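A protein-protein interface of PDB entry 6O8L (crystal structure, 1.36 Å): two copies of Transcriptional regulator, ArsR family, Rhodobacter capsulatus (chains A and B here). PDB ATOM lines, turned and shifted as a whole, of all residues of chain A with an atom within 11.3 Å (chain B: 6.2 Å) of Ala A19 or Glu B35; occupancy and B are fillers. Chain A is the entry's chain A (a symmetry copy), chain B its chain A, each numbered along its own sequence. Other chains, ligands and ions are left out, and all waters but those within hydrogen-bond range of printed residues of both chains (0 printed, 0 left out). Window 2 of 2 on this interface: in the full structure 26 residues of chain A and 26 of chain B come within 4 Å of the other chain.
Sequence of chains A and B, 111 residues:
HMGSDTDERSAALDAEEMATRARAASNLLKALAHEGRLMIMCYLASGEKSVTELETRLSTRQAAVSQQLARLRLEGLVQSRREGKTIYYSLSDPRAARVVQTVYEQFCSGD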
ATOM      1  N   ALA A  19      22.540  23.174  15.710  1.00  0.00           N
ATOM      2  CA  ALA A  19      23.279  22.135  14.997  1.00  0.00           C
ATOM      3  C   ALA A  19      24.604  22.685  14.484  1.00  0.00           C
ATOM      4  O   ALA A  19      25.640  22.024  14.588  1.00  0.00           O
ATOM      5  CB  ALA A  19      22.461  21.583  13.840  1.00  0.00           C
ATOM      6  N   THR A  20      24.565  23.896  13.922  1.00  0.00           N
ATOM      7  CA  THR A  20      25.796  24.543  13.473  1.00  0.00           C
ATOM      8  C   THR A  20      26.718  24.817  14.653  1.00  0.00           C
ATOM      9  O   THR A  20      27.924  24.546  14.597  1.00  0.00           O
ATOM     10  CB  THR A  20      25.465  25.836  12.729  1.00  0.00           C
ATOM     11  OG1 THR A  20      25.037  26.837  13.664  1.00  0.00           O
ATOM     12  CG2 THR A  20      24.364  25.597  11.704  1.00  0.00           C
ATOM     13  N   ARG A  21      26.167  25.352  15.741  1.00  0.00           N
ATOM     14  CA  ARG A  21      26.964  25.501  16.950  1.00  0.00           C
ATOM     15  C   ARG A  21      27.458  24.150  17.448  1.00  0.00           C
ATOM     16  O   ARG A  21      28.536  24.068  18.047  1.00  0.00           O
ATOM     17  CB  ARG A  21      26.140  26.193  18.034  1.00  0.00           C
ATOM     18  CG  ARG A  21      25.437  27.472  17.580  1.00  0.00           C
ATOM     19  CD  ARG A  21      26.418  28.488  17.005  1.00  0.00           C
ATOM     20  NE  ARG A  21      26.433  29.742  17.761  1.00  0.00           N
ATOM     21  CZ  ARG A  21      26.952  30.883  17.313  1.00  0.00           C
ATOM     22  NH1 ARG A  21      27.495  30.939  16.107  1.00  0.00           N
ATOM     23  NH2 ARG A  21      26.927  31.974  18.070  1.00  0.00           N
ATOM     24  N   ALA A  22      26.695  23.080  17.195  1.00  0.00           N
ATOM     25  CA  ALA A  22      27.086  21.753  17.666  1.00  0.00           C
ATOM     26  C   ALA A  22      28.306  21.227  16.922  1.00  0.00           C
ATOM     27  O   ALA A  22      29.169  20.568  17.522  1.00  0.00           O
ATOM     28  CB  ALA A  22      25.931  20.768  17.494  1.00  0.00           C
ATOM     29  N   ARG A  23      28.362  21.445  15.604  1.00  0.00           N
ATOM     30  CA  ARG A  23      29.531  21.037  14.832  1.00  0.00           C
ATOM     31  C   ARG A  23      30.772  21.761  15.334  1.00  0.00           C
ATOM     32  O   ARG A  23      31.817  21.142  15.562  1.00  0.00           O
ATOM     33  CB  ARG A  23      29.296  21.313  13.345  1.00  0.00           C
ATOM     34  CG  ARG A  23      30.482  20.974  12.455  1.00  0.00           C
ATOM     35  CD  ARG A  23      30.447  19.522  11.983  1.00  0.00           C
ATOM     36  NE  ARG A  23      31.788  18.946  11.872  1.00  0.00           N
ATOM     37  CZ  ARG A  23      32.069  17.803  11.249  1.00  0.00           C
ATOM     38  NH1 ARG A  23      31.102  17.097  10.675  1.00  0.00           N
ATOM     39  NH2 ARG A  23      33.322  17.363  11.199  1.00  0.00           N
ATOM     40  N   ALA A  24      30.661  23.075  15.543  1.00  0.00           N
ATOM     41  CA  ALA A  24      31.789  23.854  16.037  1.00  0.00           C
ATOM     42  C   ALA A  24      32.217  23.381  17.420  1.00  0.00           C
ATOM     43  O   ALA A  24      33.407  23.168  17.680  1.00  0.00           O
ATOM     44  CB  ALA A  24      31.412  25.337  16.068  1.00  0.00           C
ATOM     45  N   ALA A  25      31.254  23.214  18.326  1.00  0.00           N
ATOM     46  CA  ALA A  25      31.579  22.748  19.666  1.00  0.00           C
ATOM     47  C   ALA A  25      32.173  21.345  19.629  1.00  0.00           C
ATOM     48  O   ALA A  25      33.132  21.052  20.350  1.00  0.00           O
ATOM     49  CB  ALA A  25      30.325  22.784  20.537  1.00  0.00           C
ATOM     50  N   SER A  26      31.623  20.467  18.786  1.00  0.00           N
ATOM     51  CA  SER A  26      32.125  19.098  18.709  1.00  0.00           C
ATOM     52  C   SER A  26      33.575  19.073  18.241  1.00  0.00           C
ATOM     53  O   SER A  26      34.379  18.253  18.709  1.00  0.00           O
ATOM     54  CB  SER A  26      31.237  18.283  17.771  1.00  0.00           C
ATOM     55  OG  SER A  26      31.861  17.062  17.432  1.00  0.00           O
ATOM     56  N   ASN A  27      33.936  19.975  17.331  1.00  0.00           N
ATOM     57  CA  ASN A  27      35.320  20.023  16.877  1.00  0.00           C
ATOM     58  C   ASN A  27      36.251  20.476  17.991  1.00  0.00           C
ATOM     59  O   ASN A  27      37.366  19.959  18.113  1.00  0.00           O
ATOM     60  CB  ASN A  27      35.447  20.903  15.640  1.00  0.00           C
ATOM     61  CG  ASN A  27      35.006  20.187  14.371  1.00  0.00           C
ATOM     62  OD1 ASN A  27      34.857  18.959  14.345  1.00  0.00           O
ATOM     63  ND2 ASN A  27      34.783  20.955  13.319  1.00  0.00           N
ATOM     64  N   LEU A  28      35.816  21.424  18.827  1.00  0.00           N
ATOM     65  CA  LEU A  28      36.615  21.776  19.998  1.00  0.00           C
ATOM     66  C   LEU A  28      36.788  20.569  20.904  1.00  0.00           C
ATOM     67  O   LEU A  28      37.900  20.258  21.351  1.00  0.00           O
ATOM     68  CB  LEU A  28      35.958  22.911  20.778  1.00  0.00           C
ATOM     69  CG  LEU A  28      36.595  23.160  22.153  1.00  0.00           C
ATOM     70  CD1 LEU A  28      38.089  23.554  22.040  1.00  0.00           C
ATOM     71  CD2 LEU A  28      35.803  24.206  22.910  1.00  0.00           C
ATOM     72  N   LEU A  29      35.691  19.866  21.176  1.00  0.00           N
ATOM     73  CA  LEU A  29      35.767  18.744  22.094  1.00  0.00           C
ATOM     74  C   LEU A  29      36.651  17.637  21.541  1.00  0.00           C
ATOM     75  O   LEU A  29      37.345  16.973  22.311  1.00  0.00           O
ATOM     76  CB  LEU A  29      34.358  18.275  22.454  1.00  0.00           C
ATOM     77  CG  LEU A  29      33.490  19.334  23.157  1.00  0.00           C
ATOM     78  CD1 LEU A  29      32.129  18.734  23.452  1.00  0.00           C
ATOM     79  CD2 LEU A  29      34.126  19.841  24.419  1.00  0.00           C
ATOM     80  N   LYS A  30      36.712  17.485  20.214  1.00  0.00           N
ATOM     81  CA  LYS A  30      37.631  16.511  19.626  1.00  0.00           C
ATOM     82  C   LYS A  30      39.079  16.903  19.870  1.00  0.00           C
ATOM     83  O   LYS A  30      39.923  16.045  20.151  1.00  0.00           O
ATOM     84  CB  LYS A  30      37.356  16.372  18.132  1.00  0.00           C
ATOM     85  CG  LYS A  30      36.086  15.615  17.846  1.00  0.00           C
ATOM     86  CD  LYS A  30      35.769  15.568  16.368  1.00  0.00           C
ATOM     87  CE  LYS A  30      34.464  14.820  16.117  1.00  0.00           C
ATOM     88  NZ  LYS A  30      33.953  15.011  14.727  1.00  0.00           N
ATOM     89  N   LEU B  32      31.241  13.298  24.511  1.00  0.00           N
ATOM     90  CA  LEU B  32      30.604  14.541  24.088  1.00  0.00           C
ATOM     91  C   LEU B  32      31.040  15.008  22.704  1.00  0.00           C
ATOM     92  O   LEU B  32      30.347  15.845  22.107  1.00  0.00           O
ATOM     93  CB  LEU B  32      30.887  15.662  25.084  1.00  0.00           C
ATOM     94  CG  LEU B  32      30.425  15.407  26.514  1.00  0.00           C
ATOM     95  CD1 LEU B  32      30.844  16.556  27.407  1.00  0.00           C
ATOM     96  CD2 LEU B  32      28.911  15.215  26.559  1.00  0.00           C
ATOM     97  N   ALA B  33      32.135  14.472  22.168  1.00  0.00           N
ATOM     98  CA  ALA B  33      32.733  14.968  20.927  1.00  0.00           C
ATOM     99  C   ALA B  33      32.122  14.270  19.713  1.00  0.00           C
ATOM    100  O   ALA B  33      32.778  13.560  18.950  1.00  0.00           O
ATOM    101  CB  ALA B  33      34.240  14.777  20.966  1.00  0.00           C
ATOM    102  N   HIS B  34      30.835  14.513  19.560  1.00  0.00           N
ATOM    103  CA  HIS B  34      29.991  13.830  18.594  1.00  0.00           C
ATOM    104  C   HIS B  34      28.784  14.740  18.479  1.00  0.00           C
ATOM    105  O   HIS B  34      28.143  15.048  19.489  1.00  0.00           O
ATOM    106  CB  HIS B  34      29.583  12.454  19.104  1.00  0.00           C
ATOM    107  CG  HIS B  34      28.715  11.698  18.155  1.00  0.00           C
ATOM    108  ND1 HIS B  34      27.359  11.917  18.050  1.00  0.00           N
ATOM    109  CD2 HIS B  34      29.012  10.733  17.257  1.00  0.00           C
ATOM    110  CE1 HIS B  34      26.857  11.110  17.132  1.00  0.00           C
ATOM    111  NE2 HIS B  34      27.840  10.386  16.631  1.00  0.00           N
ATOM    112  N   GLU B  35      28.507  15.217  17.268  1.00  0.00           N
ATOM    113  CA  GLU B  35      27.492  16.253  17.115  1.00  0.00           C
ATOM    114  C   GLU B  35      26.147  15.787  17.654  1.00  0.00           C
ATOM    115  O   GLU B  35      25.456  16.537  18.353  1.00  0.00           O
ATOM    116  CB  GLU B  35      27.390  16.667  15.647  1.00  0.00           C
ATOM    117  CG  GLU B  35      26.396  17.788  15.378  1.00  0.00           C
ATOM    118  CD  GLU B  35      26.469  18.312  13.952  1.00  0.00           C
ATOM    119  OE1 GLU B  35      25.401  18.643  13.388  1.00  0.00           O
ATOM    120  OE2 GLU B  35      27.593  18.395  13.403  1.00  0.00           O
ATOM    121  N   GLY B  36      25.762  14.548  17.354  1.00  0.00           N
ATOM    122  CA  GLY B  36      24.450  14.077  17.764  1.00  0.00           C
ATOM    123  C   GLY B  36      24.335  13.913  19.265  1.00  0.00           C
ATOM    124  O   GLY B  36      23.364  14.363  19.881  1.00  0.00           O
ATOM    125  N   ARG B  37      25.333  13.273  19.879  1.00  0.00           N
ATOM    126  CA  ARG B  37      25.312  13.105  21.326  1.00  0.00           C
ATOM    127  C   ARG B  37      25.396  14.452  22.029  1.00  0.00           C
ATOM    128  O   ARG B  37      24.722  14.671  23.041  1.00  0.00           O
ATOM    129  CB  ARG B  37      26.444  12.180  21.763  1.00  0.00           C
ATOM    130  CG  ARG B  37      26.275  10.752  21.292  1.00  0.00           C
ATOM    131  CD  ARG B  37      27.155   9.783  22.069  1.00  0.00           C
ATOM    132  NE  ARG B  37      28.589  10.051  21.911  1.00  0.00           N
ATOM    133  CZ  ARG B  37      29.398   9.475  21.025  1.00  0.00           C
ATOM    134  NH1 ARG B  37      28.939   8.578  20.158  1.00  0.00           N
ATOM    135  NH2 ARG B  37      30.683   9.812  21.007  1.00  0.00           N
ATOM    136  N   LEU B  38      26.195  15.376  21.492  1.00  0.00           N
ATOM    137  CA  LEU B  38      26.316  16.690  22.109  1.00  0.00           C
ATOM    138  C   LEU B  38      24.996  17.446  22.054  1.00  0.00           C
ATOM    139  O   LEU B  38      24.614  18.114  23.022  1.00  0.00           O
ATOM    140  CB  LEU B  38      27.427  17.486  21.431  1.00  0.00           C
ATOM    141  CG  LEU B  38      27.668  18.895  21.977  1.00  0.00           C
ATOM    142  CD1 LEU B  38      27.996  18.836  23.464  1.00  0.00           C
ATOM    143  CD2 LEU B  38      28.763  19.587  21.183  1.00  0.00           C
ATOM    144  N   MET B  39      24.282  17.355  20.926  1.00  0.00           N
ATOM    145  CA  MET B  39      22.998  18.039  20.810  1.00  0.00           C
ATOM    146  C   MET B  39      22.010  17.528  21.847  1.00  0.00           C
ATOM    147  O   MET B  39      21.286  18.318  22.469  1.00  0.00           O
ATOM    148  CB  MET B  39      22.432  17.860  19.403  1.00  0.00           C
ATOM    149  CG  MET B  39      23.058  18.782  18.384  1.00  0.00           C
ATOM    150  SD  MET B  39      22.258  18.711  16.770  1.00  0.00           S
ATOM    151  CE  MET B  39      22.775  17.108  16.163  1.00  0.00           C
ATOM    152  N   ILE B  40      21.955  16.206  22.043  1.00  0.00           N
ATOM    153  CA  ILE B  40      21.092  15.641  23.077  1.00  0.00           C
ATOM    154  C   ILE B  40      21.455  16.231  24.429  1.00  0.00           C
ATOM    155  O   ILE B  40      20.591  16.682  25.191  1.00  0.00           O
ATOM    156  CB  ILE B  40      21.200  14.109  23.106  1.00  0.00           C
ATOM    157  CG1 ILE B  40      20.550  13.488  21.876  1.00  0.00           C
ATOM    158  CG2 ILE B  40      20.553  13.596  24.379  1.00  0.00           C
ATOM    159  CD1 ILE B  40      21.021  12.059  21.647  1.00  0.00           C
ATOM    160  N   SER B  59      17.213  16.682  14.319  1.00  0.00           N
ATOM    161  CA  SER B  59      17.089  16.233  12.936  1.00  0.00           C
ATOM    162  C   SER B  59      17.485  14.772  12.773  1.00  0.00           C
ATOM    163  O   SER B  59      17.141  14.154  11.762  1.00  0.00           O
ATOM    164  CB  SER B  59      17.977  17.092  12.033  1.00  0.00           C
ATOM    165  OG  SER B  59      19.349  16.835  12.292  1.00  0.00           O
ATOM    166  N   GLN B  68      22.445   6.858  20.448  1.00  0.00           N
ATOM    167  CA  GLN B  68      23.123   7.948  21.134  1.00  0.00           C
ATOM    168  C   GLN B  68      22.653   8.067  22.576  1.00  0.00           C
ATOM    169  O   GLN B  68      23.465   8.264  23.489  1.00  0.00           O
ATOM    170  CB  GLN B  68      22.872   9.237  20.352  1.00  0.00           C
ATOM    171  CG  GLN B  68      23.588   9.243  18.993  1.00  0.00           C
ATOM    172  CD  GLN B  68      23.087  10.295  18.031  1.00  0.00           C
ATOM    173  OE1 GLN B  68      22.346  11.199  18.411  1.00  0.00           O
ATOM    174  NE2 GLN B  68      23.485  10.174  16.767  1.00  0.00           N
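OG of Ser A26 sits at hydrogen-bond distance from N of His B34 (3.5 Å).
Of the printed residues of chain B, Ala A19 touches Glu B35 (3.6 Å) and Met B39 (3.99 Å).
Glu B35 touches four residues of chain A.
His B34 touches just one residue of chain A: Ser A26 (3.5 Å).
No residue of chain A comes within 4 Å of Gly B36.
Of the printed residues of chain A, Met B39 touches Ala A19 (3.99 Å) and Ala A22 (3.6 Å).
Printed residues of chain B within 4 Å of Lys A30: Ala B33 (3.5 Å).
Of the printed residues of chain B, Ala A25 touches Leu B38.
Of the printed residues of chain B, Arg A23 touches Glu B35 (3.4 Å).
Arg A21 touches none of the printed residues of chain B.
Gln B68 touches none of the printed residues of chain A.
The nearest printed residue of chain B that does not touch Ala A19 is Ser B59 (5.9 Å).
The nearest printed residue of chain B that does not touch Leu A29 is Leu B38 (4.1 Å).
No position is printed for both chains.
ND1 of His B34 sits at hydrogen-bond distance from N of Gly B36.
The backbone NH (N) of Arg B37 is in hydrogen-bond range of a ring nitrogen (ND1) of His B34, 3.0 Å away.
Of the 12 printed residues of chain A, 7 touch a printed residue of chain B.
Hydrophobic or aromatic side chains of chain A within 4 Å of the printed part of chain B: Ala A22, Ala A25 and Leu A29.
Of the 11 printed residues of chain B, 6 touch a printed residue of chain A.
Hydrophobic or aromatic side chains of chain B that line the printed part of chain A: Leu B32, Ala B33, Leu B38 and Met B39.
Along chain B the printed residues that touch a printed residue of chain A span positions 32 to 39.
Among the printed residues, 14 pairs touch across the chains.
O of Ala A19 touches OE1 of Glu B35 (3.6 Å).
CG of Glu B35 touches CB of Ala A22, at 3.7 Å.
Ala A22 touches Leu B38 (O to CD2, 3.8 Å).
Ala A22 touches Met B39 (CB to CG, 3.6 Å).
Arg A23 touches Glu B35.
Ala A25 touches Leu B38 (CB to CD2, 3.6 Å).
Ala B33 touches Ser A26 (C to OG, 3.6 Å).
Ser A26 touches Glu B35 (OG to N, 3.8 Å).
Ser A26 touches Leu B38.
Ala B33 touches Lys A30.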
